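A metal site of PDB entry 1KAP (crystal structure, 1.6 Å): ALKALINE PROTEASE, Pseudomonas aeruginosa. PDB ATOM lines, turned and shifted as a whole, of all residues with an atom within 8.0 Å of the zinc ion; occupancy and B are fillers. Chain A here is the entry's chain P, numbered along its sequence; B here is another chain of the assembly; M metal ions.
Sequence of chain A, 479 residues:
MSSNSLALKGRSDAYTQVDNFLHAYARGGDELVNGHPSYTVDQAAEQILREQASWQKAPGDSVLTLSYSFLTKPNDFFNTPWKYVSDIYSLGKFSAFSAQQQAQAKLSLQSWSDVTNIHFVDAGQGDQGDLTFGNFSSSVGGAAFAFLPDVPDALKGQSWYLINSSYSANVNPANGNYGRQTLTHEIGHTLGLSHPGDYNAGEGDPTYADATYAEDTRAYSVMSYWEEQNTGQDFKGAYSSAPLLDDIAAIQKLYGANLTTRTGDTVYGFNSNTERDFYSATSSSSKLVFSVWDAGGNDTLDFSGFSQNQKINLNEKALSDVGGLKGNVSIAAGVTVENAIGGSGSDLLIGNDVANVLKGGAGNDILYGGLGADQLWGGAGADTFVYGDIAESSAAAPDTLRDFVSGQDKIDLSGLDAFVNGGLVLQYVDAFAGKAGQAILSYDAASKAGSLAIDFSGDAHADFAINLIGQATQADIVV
The chain-end carboxylate (OXT) of Ser 4 of chain B sits close to the side-chain carboxylate (OE2) of Glu 186 (2.7 Å). The backbone carbonyl oxygen (O) of Val 222 sits at hydrogen-bond distance from a ring nitrogen (ND1) of His 185 (2.7 Å). The side-chain hydroxyl (OH) of Tyr 225 lies close to the chain-end carboxylate (O) of Ser 4 of chain B, 2.6 Å away. A ring nitrogen (ND1) of His 189 sits at hydrogen-bond distance from the backbone carbonyl oxygen (O) of Leu 193. A ring nitrogen (ND1) of His 195 is in hydrogen-bond range of the backbone carbonyl oxygen (O) of Tyr 199, 2.8 Å away. The backbone NH (N) of Ser 4 of chain B lies within hydrogen-bond range of the side-chain amide oxygen (OD1) of Asn 200, 2.9 Å away.
The nearest printed residue that does not touch the zinc ion is Tyr 225 (4.1 Å).
The zinc ion is bound by a ring nitrogen (NE2) of His 189 (2.1 Å), a ring nitrogen (NE2) of His 195 (2.1 Å), a ring nitrogen (NE2) of His 185 (2.1 Å), the chain-end carboxylate (O) of Ser 4 of chain B (2.2 Å) and the chain-end carboxylate (OXT) of Ser 4 of chain B (2.5 Å).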
ATOM      1  N   ALA A 144       6.589   6.126  15.397  1.00  0.00           N
ATOM      2  CA  ALA A 144       5.223   5.638  15.415  1.00  0.00           C
ATOM      3  C   ALA A 144       5.201   4.326  16.179  1.00  0.00           C
ATOM      4  O   ALA A 144       6.247   3.791  16.510  1.00  0.00           O
ATOM      5  CB  ALA A 144       4.722   5.417  13.980  1.00  0.00           C
ATOM      6  N   PHE A 145       4.013   3.830  16.490  1.00  0.00           N
ATOM      7  CA  PHE A 145       3.890   2.564  17.187  1.00  0.00           C
ATOM      8  C   PHE A 145       2.532   1.913  16.895  1.00  0.00           C
ATOM      9  O   PHE A 145       1.611   2.567  16.391  1.00  0.00           O
ATOM     10  CB  PHE A 145       4.148   2.704  18.698  1.00  0.00           C
ATOM     11  CG  PHE A 145       3.127   3.562  19.433  1.00  0.00           C
ATOM     12  CD1 PHE A 145       1.944   3.002  19.902  1.00  0.00           C
ATOM     13  CD2 PHE A 145       3.380   4.921  19.661  1.00  0.00           C
ATOM     14  CE1 PHE A 145       1.011   3.788  20.593  1.00  0.00           C
ATOM     15  CE2 PHE A 145       2.459   5.714  20.350  1.00  0.00           C
ATOM     16  CZ  PHE A 145       1.273   5.145  20.822  1.00  0.00           C
ATOM     17  N   ALA A 146       2.442   0.626  17.165  1.00  0.00           N
ATOM     18  CA  ALA A 146       1.217  -0.120  16.936  1.00  0.00           C
ATOM     19  C   ALA A 146       1.167  -1.279  17.900  1.00  0.00           C
ATOM     20  O   ALA A 146       2.116  -1.524  18.648  1.00  0.00           O
ATOM     21  CB  ALA A 146       1.194  -0.650  15.490  1.00  0.00           C
ATOM     22  N   LEU A 148       0.175  -5.490  18.292  1.00  0.00           N
ATOM     23  CA  LEU A 148      -0.041  -6.778  17.614  1.00  0.00           C
ATOM     24  C   LEU A 148      -1.467  -7.201  17.988  1.00  0.00           C
ATOM     25  O   LEU A 148      -2.004  -6.737  18.996  1.00  0.00           O
ATOM     26  CB  LEU A 148       0.977  -7.823  18.092  1.00  0.00           C
ATOM     27  CG  LEU A 148       2.435  -7.926  17.561  1.00  0.00           C
ATOM     28  CD1 LEU A 148       2.584  -9.090  16.618  1.00  0.00           C
ATOM     29  CD2 LEU A 148       2.902  -6.644  16.935  1.00  0.00           C
ATOM     30  N   TYR A 178      10.356   7.621   3.789  1.00  0.00           N
ATOM     31  CA  TYR A 178      10.209   7.002   5.087  1.00  0.00           C
ATOM     32  C   TYR A 178       8.798   7.051   5.683  1.00  0.00           C
ATOM     33  O   TYR A 178       8.379   6.102   6.335  1.00  0.00           O
ATOM     34  CB  TYR A 178      11.242   7.548   6.068  1.00  0.00           C
ATOM     35  CG  TYR A 178      11.422   6.659   7.265  1.00  0.00           C
ATOM     36  CD1 TYR A 178      11.787   5.316   7.100  1.00  0.00           C
ATOM     37  CD2 TYR A 178      11.183   7.125   8.549  1.00  0.00           C
ATOM     38  CE1 TYR A 178      11.900   4.456   8.197  1.00  0.00           C
ATOM     39  CE2 TYR A 178      11.297   6.284   9.659  1.00  0.00           C
ATOM     40  CZ  TYR A 178      11.659   4.956   9.475  1.00  0.00           C
ATOM     41  OH  TYR A 178      11.769   4.116  10.561  1.00  0.00           O
ATOM     42  N   THR A 182       6.790   3.824   6.927  1.00  0.00           N
ATOM     43  CA  THR A 182       6.312   3.781   8.314  1.00  0.00           C
ATOM     44  C   THR A 182       4.850   3.295   8.391  1.00  0.00           C
ATOM     45  O   THR A 182       4.513   2.466   9.225  1.00  0.00           O
ATOM     46  CB  THR A 182       6.493   5.173   9.015  1.00  0.00           C
ATOM     47  OG1 THR A 182       7.886   5.445   9.143  1.00  0.00           O
ATOM     48  CG2 THR A 182       5.852   5.193  10.399  1.00  0.00           C
ATOM     49  N   HIS A 185       4.860  -0.429   7.611  1.00  0.00           N
ATOM     50  CA  HIS A 185       5.488  -1.103   8.741  1.00  0.00           C
ATOM     51  C   HIS A 185       4.501  -1.227   9.929  1.00  0.00           C
ATOM     52  O   HIS A 185       4.302  -2.326  10.465  1.00  0.00           O
ATOM     53  CB  HIS A 185       6.733  -0.314   9.120  1.00  0.00           C
ATOM     54  CG  HIS A 185       7.455  -0.818  10.329  1.00  0.00           C
ATOM     55  ND1 HIS A 185       8.680  -1.442  10.260  1.00  0.00           N
ATOM     56  CD2 HIS A 185       7.161  -0.710  11.646  1.00  0.00           C
ATOM     57  CE1 HIS A 185       9.110  -1.696  11.482  1.00  0.00           C
ATOM     58  NE2 HIS A 185       8.212  -1.255  12.343  1.00  0.00           N
ATOM     59  N   GLU A 186       3.857  -0.122  10.326  1.00  0.00           N
ATOM     60  CA  GLU A 186       2.912  -0.167  11.444  1.00  0.00           C
ATOM     61  C   GLU A 186       1.710  -1.049  11.162  1.00  0.00           C
ATOM     62  O   GLU A 186       1.270  -1.797  12.024  1.00  0.00           O
ATOM     63  CB  GLU A 186       2.471   1.223  11.871  1.00  0.00           C
ATOM     64  CG  GLU A 186       3.597   2.132  12.346  1.00  0.00           C
ATOM     65  CD  GLU A 186       4.464   1.539  13.468  1.00  0.00           C
ATOM     66  OE1 GLU A 186       4.007   0.692  14.256  1.00  0.00           O
ATOM     67  OE2 GLU A 186       5.642   1.946  13.564  1.00  0.00           O
ATOM     68  N   GLY A 188       1.770  -3.573   9.262  1.00  0.00           N
ATOM     69  CA  GLY A 188       2.279  -4.940   9.382  1.00  0.00           C
ATOM     70  C   GLY A 188       2.160  -5.423  10.839  1.00  0.00           C
ATOM     71  O   GLY A 188       1.756  -6.554  11.078  1.00  0.00           O
ATOM     72  N   HIS A 189       2.515  -4.565  11.797  1.00  0.00           N
ATOM     73  CA  HIS A 189       2.398  -4.924  13.223  1.00  0.00           C
ATOM     74  C   HIS A 189       0.943  -5.231  13.604  1.00  0.00           C
ATOM     75  O   HIS A 189       0.669  -6.221  14.268  1.00  0.00           O
ATOM     76  CB  HIS A 189       2.876  -3.798  14.123  1.00  0.00           C
ATOM     77  CG  HIS A 189       4.352  -3.671  14.245  1.00  0.00           C
ATOM     78  ND1 HIS A 189       5.189  -4.762  14.390  1.00  0.00           N
ATOM     79  CD2 HIS A 189       5.146  -2.581  14.301  1.00  0.00           C
ATOM     80  CE1 HIS A 189       6.430  -4.347  14.543  1.00  0.00           C
ATOM     81  NE2 HIS A 189       6.428  -3.027  14.496  1.00  0.00           N
ATOM     82  N   LEU A 193       2.706  -9.110  12.429  1.00  0.00           N
ATOM     83  CA  LEU A 193       4.133  -9.230  12.176  1.00  0.00           C
ATOM     84  C   LEU A 193       4.998  -8.501  13.204  1.00  0.00           C
ATOM     85  O   LEU A 193       4.695  -7.365  13.606  1.00  0.00           O
ATOM     86  CB  LEU A 193       4.488  -8.717  10.771  1.00  0.00           C
ATOM     87  CG  LEU A 193       3.676  -9.237   9.562  1.00  0.00           C
ATOM     88  CD1 LEU A 193       4.301  -8.721   8.272  1.00  0.00           C
ATOM     89  CD2 LEU A 193       3.633 -10.747   9.568  1.00  0.00           C
ATOM     90  N   SER A 194       6.073  -9.155  13.621  1.00  0.00           N
ATOM     91  CA  SER A 194       7.030  -8.568  14.562  1.00  0.00           C
ATOM     92  C   SER A 194       8.245  -8.086  13.764  1.00  0.00           C
ATOM     93  O   SER A 194       8.318  -8.248  12.545  1.00  0.00           O
ATOM     94  CB  SER A 194       7.505  -9.641  15.555  1.00  0.00           C
ATOM     95  OG  SER A 194       6.451 -10.063  16.394  1.00  0.00           O
ATOM     96  N   HIS A 195       9.179  -7.420  14.448  1.00  0.00           N
ATOM     97  CA  HIS A 195      10.432  -7.054  13.792  1.00  0.00           C
ATOM     98  C   HIS A 195      11.095  -8.424  13.625  1.00  0.00           C
ATOM     99  O   HIS A 195      10.762  -9.371  14.363  1.00  0.00           O
ATOM    100  CB  HIS A 195      11.310  -6.193  14.698  1.00  0.00           C
ATOM    101  CG  HIS A 195      10.710  -4.877  15.057  1.00  0.00           C
ATOM    102  ND1 HIS A 195      10.794  -4.337  16.323  1.00  0.00           N
ATOM    103  CD2 HIS A 195       9.984  -3.994  14.318  1.00  0.00           C
ATOM    104  CE1 HIS A 195      10.156  -3.184  16.345  1.00  0.00           C
ATOM    105  NE2 HIS A 195       9.654  -2.957  15.141  1.00  0.00           N
ATOM    106  N   PRO A 196      12.018  -8.561  12.666  1.00  0.00           N
ATOM    107  CA  PRO A 196      12.691  -9.850  12.435  1.00  0.00           C
ATOM    108  C   PRO A 196      13.574 -10.315  13.617  1.00  0.00           C
ATOM    109  O   PRO A 196      14.014 -11.454  13.659  1.00  0.00           O
ATOM    110  CB  PRO A 196      13.535  -9.584  11.182  1.00  0.00           C
ATOM    111  CG  PRO A 196      12.747  -8.487  10.462  1.00  0.00           C
ATOM    112  CD  PRO A 196      12.361  -7.587  11.610  1.00  0.00           C
ATOM    113  N   TYR A 199      14.160  -6.620  19.153  1.00  0.00           N
ATOM    114  CA  TYR A 199      14.633  -5.269  19.417  1.00  0.00           C
ATOM    115  C   TYR A 199      13.430  -4.354  19.192  1.00  0.00           C
ATOM    116  O   TYR A 199      12.459  -4.723  18.498  1.00  0.00           O
ATOM    117  CB  TYR A 199      15.837  -4.895  18.505  1.00  0.00           C
ATOM    118  CG  TYR A 199      15.610  -5.115  17.016  1.00  0.00           C
ATOM    119  CD1 TYR A 199      14.790  -4.267  16.286  1.00  0.00           C
ATOM    120  CD2 TYR A 199      16.214  -6.192  16.341  1.00  0.00           C
ATOM    121  CE1 TYR A 199      14.558  -4.461  14.941  1.00  0.00           C
ATOM    122  CE2 TYR A 199      15.994  -6.397  14.981  1.00  0.00           C
ATOM    123  CZ  TYR A 199      15.161  -5.529  14.284  1.00  0.00           C
ATOM    124  OH  TYR A 199      14.919  -5.675  12.937  1.00  0.00           O
ATOM    125  N   ASN A 200      13.464  -3.185  19.812  1.00  0.00           N
ATOM    126  CA  ASN A 200      12.360  -2.266  19.662  1.00  0.00           C
ATOM    127  C   ASN A 200      12.875  -0.908  20.085  1.00  0.00           C
ATOM    128  O   ASN A 200      13.759  -0.825  20.940  1.00  0.00           O
ATOM    129  CB  ASN A 200      11.197  -2.707  20.557  1.00  0.00           C
ATOM    130  CG  ASN A 200       9.930  -1.928  20.294  1.00  0.00           C
ATOM    131  OD1 ASN A 200       9.640  -1.574  19.158  1.00  0.00           O
ATOM    132  ND2 ASN A 200       9.161  -1.671  21.341  1.00  0.00           N
ATOM    133  N   ALA A 201      12.374   0.148  19.447  1.00  0.00           N
ATOM    134  CA  ALA A 201      12.808   1.497  19.799  1.00  0.00           C
ATOM    135  C   ALA A 201      12.446   1.721  21.263  1.00  0.00           C
ATOM    136  O   ALA A 201      11.398   1.256  21.730  1.00  0.00           O
ATOM    137  CB  ALA A 201      12.126   2.534  18.906  1.00  0.00           C
ATOM    138  N   VAL A 222      10.252  -4.748   5.363  1.00  0.00           N
ATOM    139  CA  VAL A 222       9.916  -3.404   5.790  1.00  0.00           C
ATOM    140  C   VAL A 222       9.763  -3.400   7.320  1.00  0.00           C
ATOM    141  O   VAL A 222       9.628  -2.341   7.935  1.00  0.00           O
ATOM    142  CB  VAL A 222       8.633  -2.837   5.126  1.00  0.00           C
ATOM    143  CG1 VAL A 222       8.828  -2.708   3.634  1.00  0.00           C
ATOM    144  CG2 VAL A 222       7.413  -3.675   5.475  1.00  0.00           C
ATOM    145  N   MET A 223       9.760  -4.585   7.930  1.00  0.00           N
ATOM    146  CA  MET A 223       9.644  -4.721   9.388  1.00  0.00           C
ATOM    147  C   MET A 223      11.011  -4.551  10.075  1.00  0.00           C
ATOM    148  O   MET A 223      11.079  -4.451  11.306  1.00  0.00           O
ATOM    149  CB  MET A 223       9.043  -6.069   9.788  1.00  0.00           C
ATOM    150  CG  MET A 223       7.671  -6.345   9.211  1.00  0.00           C
ATOM    151  SD  MET A 223       6.502  -4.998   9.422  1.00  0.00           S
ATOM    152  CE  MET A 223       6.360  -4.924  11.177  1.00  0.00           C
ATOM    153  N   SER A 224      12.082  -4.531   9.276  1.00  0.00           N
ATOM    154  CA  SER A 224      13.431  -4.368   9.795  1.00  0.00           C
ATOM    155  C   SER A 224      13.742  -2.890  10.069  1.00  0.00           C
ATOM    156  O   SER A 224      13.159  -1.990   9.459  1.00  0.00           O
ATOM    157  CB  SER A 224      14.453  -4.882   8.769  1.00  0.00           C
ATOM    158  OG  SER A 224      15.782  -4.648   9.205  1.00  0.00           O
ATOM    159  N   TYR A 225      14.680  -2.664  10.968  1.00  0.00           N
ATOM    160  CA  TYR A 225      15.144  -1.331  11.308  1.00  0.00           C
ATOM    161  C   TYR A 225      16.463  -1.023  10.576  1.00  0.00           C
ATOM    162  O   TYR A 225      16.878   0.134  10.517  1.00  0.00           O
ATOM    163  CB  TYR A 225      15.513  -1.270  12.802  1.00  0.00           C
ATOM    164  CG  TYR A 225      14.406  -0.989  13.793  1.00  0.00           C
ATOM    165  CD1 TYR A 225      13.063  -0.950  13.407  1.00  0.00           C
ATOM    166  CD2 TYR A 225      14.736  -0.737  15.129  1.00  0.00           C
ATOM    167  CE1 TYR A 225      12.053  -0.657  14.345  1.00  0.00           C
ATOM    168  CE2 TYR A 225      13.746  -0.453  16.061  1.00  0.00           C
ATOM    169  CZ  TYR A 225      12.412  -0.417  15.678  1.00  0.00           C
ATOM    170  OH  TYR A 225      11.463  -0.127  16.623  1.00  0.00           O
ATOM    171  N   SER B   2       3.150  -1.559  22.705  1.00  0.00           N
ATOM    172  CA  SER B   2       3.832  -0.443  22.072  1.00  0.00           C
ATOM    173  C   SER B   2       5.032  -0.973  21.274  1.00  0.00           C
ATOM    174  O   SER B   2       6.150  -1.066  21.779  1.00  0.00           O
ATOM    175  CB  SER B   2       4.264   0.626  23.086  1.00  0.00           C
ATOM    176  OG  SER B   2       4.712   1.816  22.449  1.00  0.00           O
ATOM    177  N   ASN B   3       4.750  -1.453  20.072  1.00  0.00           N
ATOM    178  CA  ASN B   3       5.804  -1.917  19.193  1.00  0.00           C
ATOM    179  C   ASN B   3       6.026  -0.750  18.263  1.00  0.00           C
ATOM    180  O   ASN B   3       5.072  -0.296  17.610  1.00  0.00           O
ATOM    181  CB  ASN B   3       5.349  -3.133  18.387  1.00  0.00           C
ATOM    182  CG  ASN B   3       5.993  -4.408  18.857  1.00  0.00           C
ATOM    183  OD1 ASN B   3       7.175  -4.649  18.597  1.00  0.00           O
ATOM    184  ND2 ASN B   3       5.216  -5.235  19.547  1.00  0.00           N
ATOM    185  N   SER B   4       7.234  -0.197  18.274  1.00  0.00           N
ATOM    186  CA  SER B   4       7.547   0.908  17.397  1.00  0.00           C
ATOM    187  C   SER B   4       7.873   0.278  16.025  1.00  0.00           C
ATOM    188  O   SER B   4       8.949  -0.336  15.880  1.00  0.00           O
ATOM    189  CB  SER B   4       8.730   1.716  17.941  1.00  0.00           C
ATOM    190  OG  SER B   4       8.421   2.257  19.235  1.00  0.00           O
ATOM    191  OXT SER B   4       6.991   0.274  15.141  1.00  0.00           O
HETATM  192 ZN    ZN M   1       8.090  -1.792  14.403  1.00  0.00          ZN
